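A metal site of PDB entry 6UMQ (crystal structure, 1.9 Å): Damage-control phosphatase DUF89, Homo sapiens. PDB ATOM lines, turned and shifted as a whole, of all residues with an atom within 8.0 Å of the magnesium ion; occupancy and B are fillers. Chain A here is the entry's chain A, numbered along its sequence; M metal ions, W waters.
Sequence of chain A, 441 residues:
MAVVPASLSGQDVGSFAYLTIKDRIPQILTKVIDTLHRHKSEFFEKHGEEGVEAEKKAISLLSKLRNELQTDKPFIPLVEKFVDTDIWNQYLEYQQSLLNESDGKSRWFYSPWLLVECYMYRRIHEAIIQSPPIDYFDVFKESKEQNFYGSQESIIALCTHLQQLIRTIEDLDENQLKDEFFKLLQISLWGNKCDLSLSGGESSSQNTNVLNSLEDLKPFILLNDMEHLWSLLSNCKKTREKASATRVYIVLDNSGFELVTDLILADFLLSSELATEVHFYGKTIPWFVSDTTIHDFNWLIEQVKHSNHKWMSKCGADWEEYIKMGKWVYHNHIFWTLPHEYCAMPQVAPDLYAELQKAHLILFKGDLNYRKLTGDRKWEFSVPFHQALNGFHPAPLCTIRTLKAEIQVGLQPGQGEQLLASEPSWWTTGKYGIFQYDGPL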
ATOM      1  N   LEU A 252       2.073  -1.066 -21.687  1.00  0.00           N
ATOM      2  CA  LEU A 252       1.141  -0.609 -20.674  1.00  0.00           C
ATOM      3  C   LEU A 252       0.885   0.895 -20.776  1.00  0.00           C
ATOM      4  O   LEU A 252       1.577   1.627 -21.507  1.00  0.00           O
ATOM      5  CB  LEU A 252       1.670  -0.969 -19.304  1.00  0.00           C
ATOM      6  CG  LEU A 252       1.798  -2.446 -18.966  1.00  0.00           C
ATOM      7  CD1 LEU A 252       2.633  -2.586 -17.727  1.00  0.00           C
ATOM      8  CD2 LEU A 252       0.445  -3.054 -18.786  1.00  0.00           C
ATOM      9  N   ASP A 253      -0.232   1.313 -20.161  1.00  0.00           N
ATOM     10  CA  ASP A 253      -0.567   2.718 -19.936  1.00  0.00           C
ATOM     11  C   ASP A 253      -0.709   2.922 -18.428  1.00  0.00           C
ATOM     12  O   ASP A 253       0.302   2.883 -17.732  1.00  0.00           O
ATOM     13  CB  ASP A 253      -1.830   3.099 -20.686  1.00  0.00           C
ATOM     14  CG  ASP A 253      -2.115   4.590 -20.693  1.00  0.00           C
ATOM     15  OD1 ASP A 253      -1.407   5.396 -20.043  1.00  0.00           O
ATOM     16  OD2 ASP A 253      -3.103   4.944 -21.367  1.00  0.00           O
ATOM     17  N   ASN A 254      -1.924   3.101 -17.911  1.00  0.00           N
ATOM     18  CA  ASN A 254      -2.014   3.588 -16.542  1.00  0.00           C
ATOM     19  C   ASN A 254      -1.899   2.476 -15.500  1.00  0.00           C
ATOM     20  O   ASN A 254      -2.043   1.286 -15.799  1.00  0.00           O
ATOM     21  CB  ASN A 254      -3.311   4.333 -16.346  1.00  0.00           C
ATOM     22  CG  ASN A 254      -3.350   5.599 -17.099  1.00  0.00           C
ATOM     23  OD1 ASN A 254      -2.380   6.104 -17.489  1.00  0.00           O
ATOM     24  ND2 ASN A 254      -4.545   6.099 -17.316  1.00  0.00           N
ATOM     25  N   SER A 255      -1.596   2.891 -14.277  1.00  0.00           N
ATOM     26  CA  SER A 255      -1.476   2.003 -13.129  1.00  0.00           C
ATOM     27  C   SER A 255      -2.880   1.795 -12.530  1.00  0.00           C
ATOM     28  O   SER A 255      -3.879   2.086 -13.162  1.00  0.00           O
ATOM     29  CB  SER A 255      -0.457   2.605 -12.156  1.00  0.00           C
ATOM     30  OG  SER A 255      -0.920   3.909 -11.812  1.00  0.00           O
ATOM     31  N   GLU A 258      -6.637   0.212 -14.316  1.00  0.00           N
ATOM     32  CA  GLU A 258      -6.266  -0.135 -15.682  1.00  0.00           C
ATOM     33  C   GLU A 258      -5.235  -1.247 -15.695  1.00  0.00           C
ATOM     34  O   GLU A 258      -5.346  -2.206 -16.479  1.00  0.00           O
ATOM     35  CB  GLU A 258      -5.734   1.055 -16.490  1.00  0.00           C
ATOM     36  CG  GLU A 258      -5.377   0.521 -17.918  1.00  0.00           C
ATOM     37  CD  GLU A 258      -4.908   1.541 -18.965  1.00  0.00           C
ATOM     38  OE1 GLU A 258      -4.760   1.104 -20.145  1.00  0.00           O
ATOM     39  OE2 GLU A 258      -4.670   2.721 -18.640  1.00  0.00           O
ATOM     40  N   LYS A 283       7.039   2.132 -18.071  1.00  0.00           N
ATOM     41  CA  LYS A 283       7.841   3.353 -18.228  1.00  0.00           C
ATOM     42  C   LYS A 283       8.991   3.406 -17.216  1.00  0.00           C
ATOM     43  O   LYS A 283       8.827   3.023 -16.051  1.00  0.00           O
ATOM     44  CB  LYS A 283       6.980   4.598 -18.052  1.00  0.00           C
ATOM     45  CG  LYS A 283       5.687   4.614 -18.859  1.00  0.00           C
ATOM     46  CD  LYS A 283       5.976   4.594 -20.376  1.00  0.00           C
ATOM     47  CE  LYS A 283       4.617   4.723 -21.130  1.00  0.00           C
ATOM     48  NZ  LYS A 283       3.798   3.415 -21.026  1.00  0.00           N
ATOM     49  N   TRP A 287       5.609   9.329 -15.450  1.00  0.00           N
ATOM     50  CA  TRP A 287       5.268   9.708 -16.825  1.00  0.00           C
ATOM     51  C   TRP A 287       3.769   9.906 -16.985  1.00  0.00           C
ATOM     52  O   TRP A 287       2.963   9.024 -16.617  1.00  0.00           O
ATOM     53  CB  TRP A 287       5.751   8.573 -17.724  1.00  0.00           C
ATOM     54  CG  TRP A 287       5.875   8.855 -19.185  1.00  0.00           C
ATOM     55  CD1 TRP A 287       5.163   8.285 -20.188  1.00  0.00           C
ATOM     56  CD2 TRP A 287       6.833   9.723 -19.804  1.00  0.00           C
ATOM     57  NE1 TRP A 287       5.601   8.753 -21.398  1.00  0.00           N
ATOM     58  CE2 TRP A 287       6.642   9.627 -21.184  1.00  0.00           C
ATOM     59  CE3 TRP A 287       7.822  10.564 -19.303  1.00  0.00           C
ATOM     60  CZ2 TRP A 287       7.377  10.352 -22.085  1.00  0.00           C
ATOM     61  CZ3 TRP A 287       8.574  11.285 -20.189  1.00  0.00           C
ATOM     62  CH2 TRP A 287       8.359  11.162 -21.571  1.00  0.00           C
ATOM     63  N   PHE A 288       3.388  11.048 -17.531  1.00  0.00           N
ATOM     64  CA  PHE A 288       1.991  11.327 -17.894  1.00  0.00           C
ATOM     65  C   PHE A 288       1.056  11.033 -16.743  1.00  0.00           C
ATOM     66  O   PHE A 288      -0.074  10.565 -16.914  1.00  0.00           O
ATOM     67  CB  PHE A 288       1.602  10.570 -19.150  1.00  0.00           C
ATOM     68  CG  PHE A 288       2.111  11.261 -20.428  1.00  0.00           C
ATOM     69  CD1 PHE A 288       3.447  11.217 -20.772  1.00  0.00           C
ATOM     70  CD2 PHE A 288       1.279  12.033 -21.206  1.00  0.00           C
ATOM     71  CE1 PHE A 288       3.903  11.885 -21.885  1.00  0.00           C
ATOM     72  CE2 PHE A 288       1.746  12.683 -22.341  1.00  0.00           C
ATOM     73  CZ  PHE A 288       3.015  12.588 -22.677  1.00  0.00           C
ATOM     74  N   VAL A 289       1.523  11.421 -15.557  1.00  0.00           N
ATOM     75  CA  VAL A 289       0.891  11.239 -14.267  1.00  0.00           C
ATOM     76  C   VAL A 289       0.783   9.768 -13.908  1.00  0.00           C
ATOM     77  O   VAL A 289       1.544   9.281 -13.076  1.00  0.00           O
ATOM     78  CB  VAL A 289      -0.484  11.934 -14.209  1.00  0.00           C
ATOM     79  CG1 VAL A 289      -1.089  11.737 -12.843  1.00  0.00           C
ATOM     80  CG2 VAL A 289      -0.314  13.427 -14.492  1.00  0.00           C
ATOM     81  N   SER A 290      -0.156   9.055 -14.535  1.00  0.00           N
ATOM     82  CA  SER A 290      -0.598   7.730 -14.081  1.00  0.00           C
ATOM     83  C   SER A 290       0.170   6.537 -14.643  1.00  0.00           C
ATOM     84  O   SER A 290      -0.099   5.397 -14.216  1.00  0.00           O
ATOM     85  CB  SER A 290      -2.108   7.552 -14.463  1.00  0.00           C
ATOM     86  OG  SER A 290      -2.860   8.562 -13.840  1.00  0.00           O
ATOM     87  N   ASP A 291       1.097   6.740 -15.564  1.00  0.00           N
ATOM     88  CA  ASP A 291       1.579   5.603 -16.328  1.00  0.00           C
ATOM     89  C   ASP A 291       2.470   4.713 -15.459  1.00  0.00           C
ATOM     90  O   ASP A 291       3.226   5.182 -14.623  1.00  0.00           O
ATOM     91  CB  ASP A 291       2.326   6.067 -17.576  1.00  0.00           C
ATOM     92  CG  ASP A 291       1.359   6.622 -18.644  1.00  0.00           C
ATOM     93  OD1 ASP A 291       0.206   6.900 -18.292  1.00  0.00           O
ATOM     94  OD2 ASP A 291       1.710   6.793 -19.820  1.00  0.00           O
ATOM     95  N   THR A 292       2.293   3.435 -15.647  1.00  0.00           N
ATOM     96  CA  THR A 292       2.902   2.395 -14.840  1.00  0.00           C
ATOM     97  C   THR A 292       4.405   2.362 -15.030  1.00  0.00           C
ATOM     98  O   THR A 292       4.866   2.116 -16.136  1.00  0.00           O
ATOM     99  CB  THR A 292       2.331   1.042 -15.252  1.00  0.00           C
ATOM    100  OG1 THR A 292       0.915   1.066 -15.069  1.00  0.00           O
ATOM    101  CG2 THR A 292       2.974  -0.122 -14.420  1.00  0.00           C
ATOM    102  N   LYS A 365      -1.656  -0.268 -25.076  1.00  0.00           N
ATOM    103  CA  LYS A 365      -2.743   0.313 -24.321  1.00  0.00           C
ATOM    104  C   LYS A 365      -2.752   1.831 -24.388  1.00  0.00           C
ATOM    105  O   LYS A 365      -1.722   2.446 -24.227  1.00  0.00           O
ATOM    106  CB  LYS A 365      -2.678  -0.104 -22.835  1.00  0.00           C
ATOM    107  CG  LYS A 365      -2.902  -1.599 -22.587  1.00  0.00           C
ATOM    108  CD  LYS A 365      -4.155  -2.159 -23.142  1.00  0.00           C
ATOM    109  CE  LYS A 365      -5.423  -1.482 -22.552  1.00  0.00           C
ATOM    110  NZ  LYS A 365      -5.576  -1.567 -21.091  1.00  0.00           N
ATOM    111  N   GLY A 366      -3.932   2.424 -24.635  1.00  0.00           N
ATOM    112  CA  GLY A 366      -4.152   3.826 -24.334  1.00  0.00           C
ATOM    113  C   GLY A 366      -3.777   4.849 -25.396  1.00  0.00           C
ATOM    114  O   GLY A 366      -3.182   4.564 -26.461  1.00  0.00           O
ATOM    115  N   ASP A 367      -4.144   6.101 -25.062  1.00  0.00           N
ATOM    116  CA  ASP A 367      -4.102   7.184 -26.038  1.00  0.00           C
ATOM    117  C   ASP A 367      -2.671   7.590 -26.395  1.00  0.00           C
ATOM    118  O   ASP A 367      -2.372   7.816 -27.577  1.00  0.00           O
ATOM    119  CB  ASP A 367      -4.948   8.365 -25.537  1.00  0.00           C
ATOM    120  CG  ASP A 367      -5.190   9.379 -26.596  1.00  0.00           C
ATOM    121  OD1 ASP A 367      -6.142   9.210 -27.447  1.00  0.00           O
ATOM    122  OD2 ASP A 367      -4.436  10.387 -26.565  1.00  0.00           O
ATOM    123  N   LEU A 368      -1.769   7.689 -25.430  1.00  0.00           N
ATOM    124  CA  LEU A 368      -0.387   8.081 -25.753  1.00  0.00           C
ATOM    125  C   LEU A 368       0.278   7.082 -26.670  1.00  0.00           C
ATOM    126  O   LEU A 368       0.997   7.473 -27.607  1.00  0.00           O
ATOM    127  CB  LEU A 368       0.446   8.243 -24.475  1.00  0.00           C
ATOM    128  CG  LEU A 368       1.875   8.711 -24.694  1.00  0.00           C
ATOM    129  CD1 LEU A 368       1.914  10.046 -25.467  1.00  0.00           C
ATOM    130  CD2 LEU A 368       2.623   8.872 -23.356  1.00  0.00           C
ATOM    131  N   ASN A 369       0.076   5.773 -26.422  1.00  0.00           N
ATOM    132  CA  ASN A 369       0.638   4.780 -27.335  1.00  0.00           C
ATOM    133  C   ASN A 369       0.091   4.965 -28.742  1.00  0.00           C
ATOM    134  O   ASN A 369       0.825   4.819 -29.726  1.00  0.00           O
ATOM    135  CB  ASN A 369       0.366   3.376 -26.791  1.00  0.00           C
ATOM    136  CG  ASN A 369       1.430   2.958 -25.721  1.00  0.00           C
ATOM    137  OD1 ASN A 369       2.614   3.216 -25.887  1.00  0.00           O
ATOM    138  ND2 ASN A 369       0.989   2.332 -24.639  1.00  0.00           N
ATOM    139  N   LYS A 404      -8.593  10.301 -26.566  1.00  0.00           N
ATOM    140  CA  LYS A 404      -8.286  11.506 -25.799  1.00  0.00           C
ATOM    141  C   LYS A 404      -7.383  12.453 -26.570  1.00  0.00           C
ATOM    142  O   LYS A 404      -6.575  13.183 -25.974  1.00  0.00           O
ATOM    143  CB  LYS A 404      -7.649  11.115 -24.477  1.00  0.00           C
ATOM    144  CG  LYS A 404      -8.538  10.106 -23.723  1.00  0.00           C
ATOM    145  CD  LYS A 404      -8.032   9.892 -22.320  1.00  0.00           C
ATOM    146  CE  LYS A 404      -6.907   8.908 -22.338  1.00  0.00           C
ATOM    147  NZ  LYS A 404      -7.294   7.680 -21.574  1.00  0.00           N
HETATM  148 MG    MG M   1      -1.565   7.146 -19.084  1.00  0.00          MG
HETATM  149  O   HOH W   1      -1.787   8.973 -18.078  1.00  0.00           O
HETATM  150  O   HOH W   2      -3.561   7.526 -19.988  1.00  0.00           O
HETATM  151  O   HOH W   3      -0.603   8.052 -20.678  1.00  0.00           O
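Along chain A the residues within 4 Å of the magnesium ion span positions 253 to 291.
The magnesium ion is bound by OD1 of Asp 291 (2.0 Å), OD1 of Asp 253 (2.0 Å), water W3 (2.1 Å), OD1 of Asn 254 (2.1 Å), water W1 (2.1 Å) and water W2 (2.2 Å).
The magnesium ion has six donor atoms within binding distance.
Water W2 lies within hydrogen-bond range of OD2 of Asp 253 (3.0 Å) and ND2 of Asn 254 (3.2 Å).
N of Thr 292 lies within hydrogen-bond range of O of Asp 253 (2.9 Å).
The backbone NH (N) of Asn 254 sits at hydrogen-bond distance from the side-chain carboxylate (OE2) of Glu 258, 2.9 Å away.
O of Asn 254 is in hydrogen-bond range of OG1 of Thr 292 (3.1 Å).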
